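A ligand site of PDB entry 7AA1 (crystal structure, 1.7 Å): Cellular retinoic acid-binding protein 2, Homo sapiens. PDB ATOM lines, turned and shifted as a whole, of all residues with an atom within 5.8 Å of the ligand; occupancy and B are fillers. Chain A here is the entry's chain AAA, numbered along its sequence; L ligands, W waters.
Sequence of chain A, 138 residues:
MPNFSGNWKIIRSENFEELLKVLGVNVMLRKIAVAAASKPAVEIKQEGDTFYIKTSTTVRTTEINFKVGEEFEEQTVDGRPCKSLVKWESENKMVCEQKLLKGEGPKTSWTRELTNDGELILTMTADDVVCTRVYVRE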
ATOM      1  N   ILE A  10      19.299 -38.457  29.130  1.00  0.00           N
ATOM      2  CA  ILE A  10      19.473 -38.622  27.657  1.00  0.00           C
ATOM      3  C   ILE A  10      19.600 -40.118  27.329  1.00  0.00           C
ATOM      4  O   ILE A  10      20.148 -40.859  28.181  1.00  0.00           O
ATOM      5  CB  ILE A  10      20.641 -37.824  27.116  1.00  0.00           C
ATOM      6  CG1 ILE A  10      20.480 -37.670  25.608  1.00  0.00           C
ATOM      7  CG2 ILE A  10      21.980 -38.458  27.529  1.00  0.00           C
ATOM      8  CD1 ILE A  10      21.124 -36.471  25.070  1.00  0.00           C
ATOM      9  N   PHE A  16      25.190 -33.345  17.531  1.00  0.00           N
ATOM     10  CA  PHE A  16      25.492 -32.266  18.503  1.00  0.00           C
ATOM     11  C   PHE A  16      26.821 -31.591  18.123  1.00  0.00           C
ATOM     12  O   PHE A  16      26.891 -30.366  18.018  1.00  0.00           O
ATOM     13  CB  PHE A  16      25.505 -32.804  19.937  1.00  0.00           C
ATOM     14  CG  PHE A  16      25.689 -31.688  20.946  1.00  0.00           C
ATOM     15  CD1 PHE A  16      24.776 -30.642  21.003  1.00  0.00           C
ATOM     16  CD2 PHE A  16      26.802 -31.656  21.780  1.00  0.00           C
ATOM     17  CE1 PHE A  16      24.946 -29.611  21.902  1.00  0.00           C
ATOM     18  CE2 PHE A  16      26.966 -30.636  22.690  1.00  0.00           C
ATOM     19  CZ  PHE A  16      26.032 -29.625  22.764  1.00  0.00           C
ATOM     20  N   LEU A  20      27.645 -27.721  16.751  1.00  0.00           N
ATOM     21  CA  LEU A  20      28.581 -26.761  17.355  1.00  0.00           C
ATOM     22  C   LEU A  20      29.576 -26.279  16.299  1.00  0.00           C
ATOM     23  O   LEU A  20      29.969 -25.115  16.374  1.00  0.00           O
ATOM     24  CB  LEU A  20      29.292 -27.401  18.554  1.00  0.00           C
ATOM     25  CG  LEU A  20      28.410 -27.709  19.761  1.00  0.00           C
ATOM     26  CD1 LEU A  20      29.267 -28.192  20.929  1.00  0.00           C
ATOM     27  CD2 LEU A  20      27.582 -26.498  20.156  1.00  0.00           C
ATOM     28  N   VAL A  25      32.133 -23.043  17.022  1.00  0.00           N
ATOM     29  CA  VAL A  25      32.680 -23.202  18.374  1.00  0.00           C
ATOM     30  C   VAL A  25      34.085 -23.790  18.210  1.00  0.00           C
ATOM     31  O   VAL A  25      34.300 -24.769  17.432  1.00  0.00           O
ATOM     32  CB  VAL A  25      31.774 -24.072  19.253  1.00  0.00           C
ATOM     33  CG1 VAL A  25      32.429 -24.392  20.593  1.00  0.00           C
ATOM     34  CG2 VAL A  25      30.420 -23.389  19.422  1.00  0.00           C
ATOM     35  N   LEU A  29      36.769 -26.474  22.732  1.00  0.00           N
ATOM     36  CA  LEU A  29      35.521 -26.218  23.495  1.00  0.00           C
ATOM     37  C   LEU A  29      34.464 -27.188  22.985  1.00  0.00           C
ATOM     38  O   LEU A  29      33.694 -27.702  23.781  1.00  0.00           O
ATOM     39  CB  LEU A  29      35.097 -24.767  23.320  1.00  0.00           C
ATOM     40  CG  LEU A  29      36.079 -23.702  23.817  1.00  0.00           C
ATOM     41  CD1 LEU A  29      35.443 -22.316  23.820  1.00  0.00           C
ATOM     42  CD2 LEU A  29      36.647 -24.030  25.196  1.00  0.00           C
ATOM     43  N   ARG A  30      34.449 -27.486  21.676  1.00  0.00           N
ATOM     44  CA  ARG A  30      33.454 -28.463  21.150  1.00  0.00           C
ATOM     45  C   ARG A  30      33.635 -29.826  21.802  1.00  0.00           C
ATOM     46  O   ARG A  30      32.637 -30.450  22.106  1.00  0.00           O
ATOM     47  CB  ARG A  30      33.581 -28.673  19.636  1.00  0.00           C
ATOM     48  CG  ARG A  30      32.965 -27.562  18.830  1.00  0.00           C
ATOM     49  CD  ARG A  30      32.603 -28.013  17.429  1.00  0.00           C
ATOM     50  NE  ARG A  30      33.609 -28.767  16.713  1.00  0.00           N
ATOM     51  CZ  ARG A  30      34.508 -28.257  15.866  1.00  0.00           C
ATOM     52  NH1 ARG A  30      34.621 -26.947  15.677  1.00  0.00           N
ATOM     53  NH2 ARG A  30      35.324 -29.079  15.237  1.00  0.00           N
ATOM     54  N   ILE A  32      35.015 -30.603  24.734  1.00  0.00           N
ATOM     55  CA  ILE A  32      34.527 -30.500  26.132  1.00  0.00           C
ATOM     56  C   ILE A  32      32.993 -30.554  26.158  1.00  0.00           C
ATOM     57  O   ILE A  32      32.409 -31.279  26.981  1.00  0.00           O
ATOM     58  CB  ILE A  32      35.058 -29.202  26.755  1.00  0.00           C
ATOM     59  CG1 ILE A  32      36.596 -29.237  26.860  1.00  0.00           C
ATOM     60  CG2 ILE A  32      34.421 -28.960  28.130  1.00  0.00           C
ATOM     61  CD1 ILE A  32      37.174 -27.934  27.195  1.00  0.00           C
ATOM     62  N   ALA A  33      32.329 -29.745  25.329  1.00  0.00           N
ATOM     63  CA  ALA A  33      30.858 -29.673  25.336  1.00  0.00           C
ATOM     64  C   ALA A  33      30.256 -31.042  25.030  1.00  0.00           C
ATOM     65  O   ALA A  33      29.252 -31.418  25.680  1.00  0.00           O
ATOM     66  CB  ALA A  33      30.408 -28.662  24.353  1.00  0.00           C
ATOM     67  N   ALA A  36      30.505 -33.195  28.049  1.00  0.00           N
ATOM     68  CA  ALA A  36      29.558 -32.759  29.098  1.00  0.00           C
ATOM     69  C   ALA A  36      28.124 -33.176  28.731  1.00  0.00           C
ATOM     70  O   ALA A  36      27.375 -33.594  29.626  1.00  0.00           O
ATOM     71  CB  ALA A  36      29.660 -31.264  29.263  1.00  0.00           C
ATOM     72  N   ALA A  37      27.763 -32.975  27.459  1.00  0.00           N
ATOM     73  CA  ALA A  37      26.414 -33.141  26.905  1.00  0.00           C
ATOM     74  C   ALA A  37      26.044 -34.629  26.844  1.00  0.00           C
ATOM     75  O   ALA A  37      24.866 -34.932  26.602  1.00  0.00           O
ATOM     76  CB  ALA A  37      26.365 -32.556  25.519  1.00  0.00           C
ATOM     77  N   PRO A  40      23.569 -35.135  30.615  1.00  0.00           N
ATOM     78  CA  PRO A  40      22.850 -34.008  31.171  1.00  0.00           C
ATOM     79  C   PRO A  40      21.771 -34.477  32.142  1.00  0.00           C
ATOM     80  O   PRO A  40      21.339 -35.648  32.081  1.00  0.00           O
ATOM     81  CB  PRO A  40      22.229 -33.382  29.915  1.00  0.00           C
ATOM     82  CG  PRO A  40      21.924 -34.564  29.065  1.00  0.00           C
ATOM     83  CD  PRO A  40      23.070 -35.529  29.301  1.00  0.00           C
ATOM     84  N   VAL A  42      18.033 -32.865  32.891  1.00  0.00           N
ATOM     85  CA  VAL A  42      17.080 -31.837  32.398  1.00  0.00           C
ATOM     86  C   VAL A  42      15.873 -31.866  33.321  1.00  0.00           C
ATOM     87  O   VAL A  42      15.149 -32.886  33.432  1.00  0.00           O
ATOM     88  CB  VAL A  42      16.655 -32.081  30.949  1.00  0.00           C
ATOM     89  CG1 VAL A  42      15.641 -31.018  30.538  1.00  0.00           C
ATOM     90  CG2 VAL A  42      17.869 -32.132  30.034  1.00  0.00           C
ATOM     91  N   THR A  55      18.824 -27.240  32.183  1.00  0.00           N
ATOM     92  CA  THR A  55      19.686 -28.256  31.572  1.00  0.00           C
ATOM     93  C   THR A  55      21.039 -28.168  32.276  1.00  0.00           C
ATOM     94  O   THR A  55      21.723 -27.157  32.058  1.00  0.00           O
ATOM     95  CB  THR A  55      19.734 -28.031  30.056  1.00  0.00           C
ATOM     96  OG1 THR A  55      18.378 -28.171  29.580  1.00  0.00           O
ATOM     97  CG2 THR A  55      20.614 -29.056  29.404  1.00  0.00           C
ATOM     98  N   THR A  57      24.814 -29.860  33.261  1.00  0.00           N
ATOM     99  CA  THR A  57      25.910 -30.823  33.076  1.00  0.00           C
ATOM    100  C   THR A  57      26.981 -30.424  34.084  1.00  0.00           C
ATOM    101  O   THR A  57      26.831 -29.362  34.696  1.00  0.00           O
ATOM    102  CB  THR A  57      26.538 -30.810  31.683  1.00  0.00           C
ATOM    103  OG1 THR A  57      27.209 -29.568  31.542  1.00  0.00           O
ATOM    104  CG2 THR A  57      25.539 -30.996  30.553  1.00  0.00           C
ATOM    105  N   VAL A  59      29.728 -29.269  33.438  1.00  0.00           N
ATOM    106  CA  VAL A  59      30.544 -28.129  32.931  1.00  0.00           C
ATOM    107  C   VAL A  59      29.662 -26.894  32.833  1.00  0.00           C
ATOM    108  O   VAL A  59      30.169 -25.846  33.032  1.00  0.00           O
ATOM    109  CB  VAL A  59      31.264 -28.399  31.592  1.00  0.00           C
ATOM    110  CG1 VAL A  59      31.965 -29.747  31.608  1.00  0.00           C
ATOM    111  CG2 VAL A  59      30.358 -28.259  30.396  1.00  0.00           C
ATOM    112  N   ARG A  60      28.424 -27.021  32.415  1.00  0.00           N
ATOM    113  CA  ARG A  60      27.650 -25.804  32.056  1.00  0.00           C
ATOM    114  C   ARG A  60      26.196 -26.101  32.376  1.00  0.00           C
ATOM    115  O   ARG A  60      25.717 -27.193  32.068  1.00  0.00           O
ATOM    116  CB  ARG A  60      27.834 -25.429  30.582  1.00  0.00           C
ATOM    117  CG  ARG A  60      26.781 -24.517  29.980  1.00  0.00           C
ATOM    118  CD  ARG A  60      27.050 -24.129  28.548  1.00  0.00           C
ATOM    119  NE  ARG A  60      26.027 -23.262  27.938  1.00  0.00           N
ATOM    120  CZ  ARG A  60      26.054 -21.935  27.937  1.00  0.00           C
ATOM    121  NH1 ARG A  60      27.046 -21.313  28.533  1.00  0.00           N
ATOM    122  NH2 ARG A  60      25.102 -21.235  27.350  1.00  0.00           N
ATOM    123  N   VAL A  77      22.647 -22.218  21.613  1.00  0.00           N
ATOM    124  CA  VAL A  77      23.408 -23.383  22.129  1.00  0.00           C
ATOM    125  C   VAL A  77      24.913 -23.054  22.136  1.00  0.00           C
ATOM    126  O   VAL A  77      25.648 -23.706  22.909  1.00  0.00           O
ATOM    127  CB  VAL A  77      23.034 -24.622  21.293  1.00  0.00           C
ATOM    128  CG1 VAL A  77      23.428 -24.433  19.831  1.00  0.00           C
ATOM    129  CG2 VAL A  77      23.648 -25.877  21.883  1.00  0.00           C
ATOM    130  N   ASP A  78      25.405 -22.103  21.316  1.00  0.00           N
ATOM    131  CA  ASP A  78      26.827 -21.654  21.377  1.00  0.00           C
ATOM    132  C   ASP A  78      27.014 -20.507  22.382  1.00  0.00           C
ATOM    133  O   ASP A  78      28.124 -19.958  22.440  1.00  0.00           O
ATOM    134  CB  ASP A  78      27.411 -21.351  19.995  1.00  0.00           C
ATOM    135  CG  ASP A  78      26.670 -20.279  19.205  1.00  0.00           C
ATOM    136  OD1 ASP A  78      25.434 -20.325  19.223  1.00  0.00           O
ATOM    137  OD2 ASP A  78      27.353 -19.441  18.562  1.00  0.00           O
ATOM    138  N   GLY A  79      26.015 -20.147  23.181  1.00  0.00           N
ATOM    139  CA  GLY A  79      26.218 -19.232  24.313  1.00  0.00           C
ATOM    140  C   GLY A  79      25.976 -17.762  23.967  1.00  0.00           C
ATOM    141  O   GLY A  79      26.325 -16.911  24.809  1.00  0.00           O
ATOM    142  N   ARG A 112      10.742 -29.038  21.014  1.00  0.00           N
ATOM    143  CA  ARG A 112      10.604 -30.071  22.053  1.00  0.00           C
ATOM    144  C   ARG A 112       9.265 -30.770  21.861  1.00  0.00           C
ATOM    145  O   ARG A 112       8.205 -30.085  21.730  1.00  0.00           O
ATOM    146  CB  ARG A 112      10.776 -29.551  23.464  1.00  0.00           C
ATOM    147  CG  ARG A 112      12.219 -29.215  23.829  1.00  0.00           C
ATOM    148  CD  ARG A 112      12.351 -28.732  25.268  1.00  0.00           C
ATOM    149  NE  ARG A 112      13.750 -28.697  25.731  1.00  0.00           N
ATOM    150  CZ  ARG A 112      14.535 -27.635  25.691  1.00  0.00           C
ATOM    151  NH1 ARG A 112      14.130 -26.489  25.174  1.00  0.00           N
ATOM    152  NH2 ARG A 112      15.764 -27.713  26.152  1.00  0.00           N
ATOM    153  N   LEU A 122      14.211 -33.422  21.816  1.00  0.00           N
ATOM    154  CA  LEU A 122      14.758 -32.067  21.542  1.00  0.00           C
ATOM    155  C   LEU A 122      15.365 -32.059  20.141  1.00  0.00           C
ATOM    156  O   LEU A 122      16.199 -32.918  19.858  1.00  0.00           O
ATOM    157  CB  LEU A 122      15.819 -31.750  22.580  1.00  0.00           C
ATOM    158  CG  LEU A 122      16.589 -30.465  22.314  1.00  0.00           C
ATOM    159  CD1 LEU A 122      15.680 -29.253  22.372  1.00  0.00           C
ATOM    160  CD2 LEU A 122      17.761 -30.397  23.279  1.00  0.00           C
ATOM    161  N   MET A 124      17.673 -29.236  17.770  1.00  0.00           N
ATOM    162  CA  MET A 124      18.307 -27.910  17.744  1.00  0.00           C
ATOM    163  C   MET A 124      18.881 -27.755  16.350  1.00  0.00           C
ATOM    164  O   MET A 124      19.500 -28.712  15.896  1.00  0.00           O
ATOM    165  CB  MET A 124      19.416 -27.799  18.782  1.00  0.00           C
ATOM    166  CG  MET A 124      18.877 -27.790  20.184  1.00  0.00           C
ATOM    167  SD  MET A 124      20.179 -27.684  21.447  1.00  0.00           S
ATOM    168  CE  MET A 124      20.950 -29.304  21.357  1.00  0.00           C
ATOM    169  N   ARG A 133      18.022 -35.026  20.039  1.00  0.00           N
ATOM    170  CA  ARG A 133      18.288 -35.608  21.343  1.00  0.00           C
ATOM    171  C   ARG A 133      17.007 -36.160  21.928  1.00  0.00           C
ATOM    172  O   ARG A 133      15.941 -35.529  21.904  1.00  0.00           O
ATOM    173  CB  ARG A 133      18.980 -34.597  22.246  1.00  0.00           C
ATOM    174  CG  ARG A 133      20.350 -34.290  21.681  1.00  0.00           C
ATOM    175  CD  ARG A 133      21.009 -33.079  22.252  1.00  0.00           C
ATOM    176  NE  ARG A 133      21.318 -33.208  23.663  1.00  0.00           N
ATOM    177  CZ  ARG A 133      22.409 -33.775  24.202  1.00  0.00           C
ATOM    178  NH1 ARG A 133      23.286 -34.416  23.476  1.00  0.00           N
ATOM    179  NH2 ARG A 133      22.565 -33.732  25.517  1.00  0.00           N
ATOM    180  N   TYR A 135      15.272 -38.085  25.296  1.00  0.00           N
ATOM    181  CA  TYR A 135      15.344 -38.275  26.766  1.00  0.00           C
ATOM    182  C   TYR A 135      14.203 -39.121  27.270  1.00  0.00           C
ATOM    183  O   TYR A 135      13.155 -39.190  26.656  1.00  0.00           O
ATOM    184  CB  TYR A 135      15.252 -36.938  27.523  1.00  0.00           C
ATOM    185  CG  TYR A 135      16.205 -35.913  26.986  1.00  0.00           C
ATOM    186  CD1 TYR A 135      15.874 -35.186  25.853  1.00  0.00           C
ATOM    187  CD2 TYR A 135      17.326 -35.529  27.698  1.00  0.00           C
ATOM    188  CE1 TYR A 135      16.720 -34.226  25.343  1.00  0.00           C
ATOM    189  CE2 TYR A 135      18.197 -34.582  27.198  1.00  0.00           C
ATOM    190  CZ  TYR A 135      17.875 -33.908  26.030  1.00  0.00           C
ATOM    191  OH  TYR A 135      18.613 -32.917  25.456  1.00  0.00           O
HETATM  192  C1  LIG L   1      31.725 -23.634  26.252  1.00  0.00           C
HETATM  193  C2  LIG L   1      24.348 -30.023  27.238  1.00  0.00           C
HETATM  194  C3  LIG L   1      31.165 -23.761  24.842  1.00  0.00           C
HETATM  195  C4  LIG L   1      29.714 -24.243  24.828  1.00  0.00           C
HETATM  196  C5  LIG L   1      26.935 -27.693  26.545  1.00  0.00           C
HETATM  197  C6  LIG L   1      29.424 -24.821  23.435  1.00  0.00           C
HETATM  198  C7  LIG L   1      28.719 -23.107  25.065  1.00  0.00           C
HETATM  199  C8  LIG L   1      29.498 -25.336  25.871  1.00  0.00           C
HETATM  200  C9  LIG L   1      28.171 -26.997  26.636  1.00  0.00           C
HETATM  201  C10 LIG L   1      25.944 -28.331  26.446  1.00  0.00           C
HETATM  202  C11 LIG L   1      24.677 -28.970  26.372  1.00  0.00           C
HETATM  203  N1  LIG L   1      28.337 -26.033  25.794  1.00  0.00           N
HETATM  204  N2  LIG L   1      30.253 -26.702  27.704  1.00  0.00           N
HETATM  205  C12 LIG L   1      32.957 -25.843  26.640  1.00  0.00           C
HETATM  206  C13 LIG L   1      31.846 -24.548  28.486  1.00  0.00           C
HETATM  207  C14 LIG L   1      31.757 -24.961  27.015  1.00  0.00           C
HETATM  208  C15 LIG L   1      23.095 -30.587  27.165  1.00  0.00           C
HETATM  209  C16 LIG L   1      22.120 -30.062  26.306  1.00  0.00           C
HETATM  210  C17 LIG L   1      20.777 -30.677  26.247  1.00  0.00           C
HETATM  211  O1  LIG L   1      19.813 -29.940  25.980  1.00  0.00           O
HETATM  212  O2  LIG L   1      20.721 -31.925  26.514  1.00  0.00           O
HETATM  213  C18 LIG L   1      22.452 -29.018  25.450  1.00  0.00           C
HETATM  214  C19 LIG L   1      23.705 -28.454  25.524  1.00  0.00           C
HETATM  215  C20 LIG L   1      29.083 -27.332  27.600  1.00  0.00           C
HETATM  216  C21 LIG L   1      30.471 -25.719  26.815  1.00  0.00           C
HETATM  217  O   HOH W   1      25.759 -25.633  24.582  1.00  0.00           O
HETATM  218  O   HOH W   2      17.468 -29.876  27.401  1.00  0.00           O
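O2 of the ligand sits at hydrogen-bond distance from OH of Tyr 135.
An oxygen (O2) of the ligand is in salt-bridge range of the guanidinium group (NH2) of Arg 133.
The side-chain hydroxyl of Tyr 135 is in hydrogen-bond range of the guanidinium group of Arg 133.
The backbone NH (N) of Leu 122 lies within hydrogen-bond range of the backbone carbonyl oxygen (O) of Arg 133.
The guanidinium group of Arg 133 sits at hydrogen-bond distance from the backbone carbonyl oxygen of Ala 37 (2.8 Å).
N of Val 59 lies close to OG1 of Thr 57, 3.2 Å away.
O of Arg 60 is in hydrogen-bond range of OG1 of Thr 57 (2.9 Å).
Phe 16 touches the ligand (CZ to C19, 3.8 Å).
O of Leu 29 touches C12 of the ligand, 3.5 Å away.
Ile 32 touches the ligand (CG2 to C12, 3.8 Å).
Ala 33 touches the ligand.
Ala 37 touches the ligand.
CG of Pro 40 touches O2 of the ligand, 3.9 Å away.
Thr 55 touches the ligand.
CG2 of Thr 57 touches C2 of the ligand, 3.7 Å away.
Val 59 touches the ligand (CG2 to N2, 3.1 Å).
Arg 60 touches the ligand.
Val 77 touches the ligand.
Leu 122 touches the ligand (CD2 to O1, 3.4 Å).
Hydrophobic or aromatic side chains that line the ligand: Phe 16, Ile 32, Ala 33, Ala 37, Pro 40, Val 59, Leu 122 and Tyr 135.
Water W2 lies within hydrogen-bond range of O1 of the ligand (2.7 Å), OG1 of Thr 55 (2.9 Å) and NH2 of Arg 112 (3.0 Å).
Water W1 lies within hydrogen-bond range of O of Val 77 (2.6 Å) and N1 of the ligand (2.9 Å).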
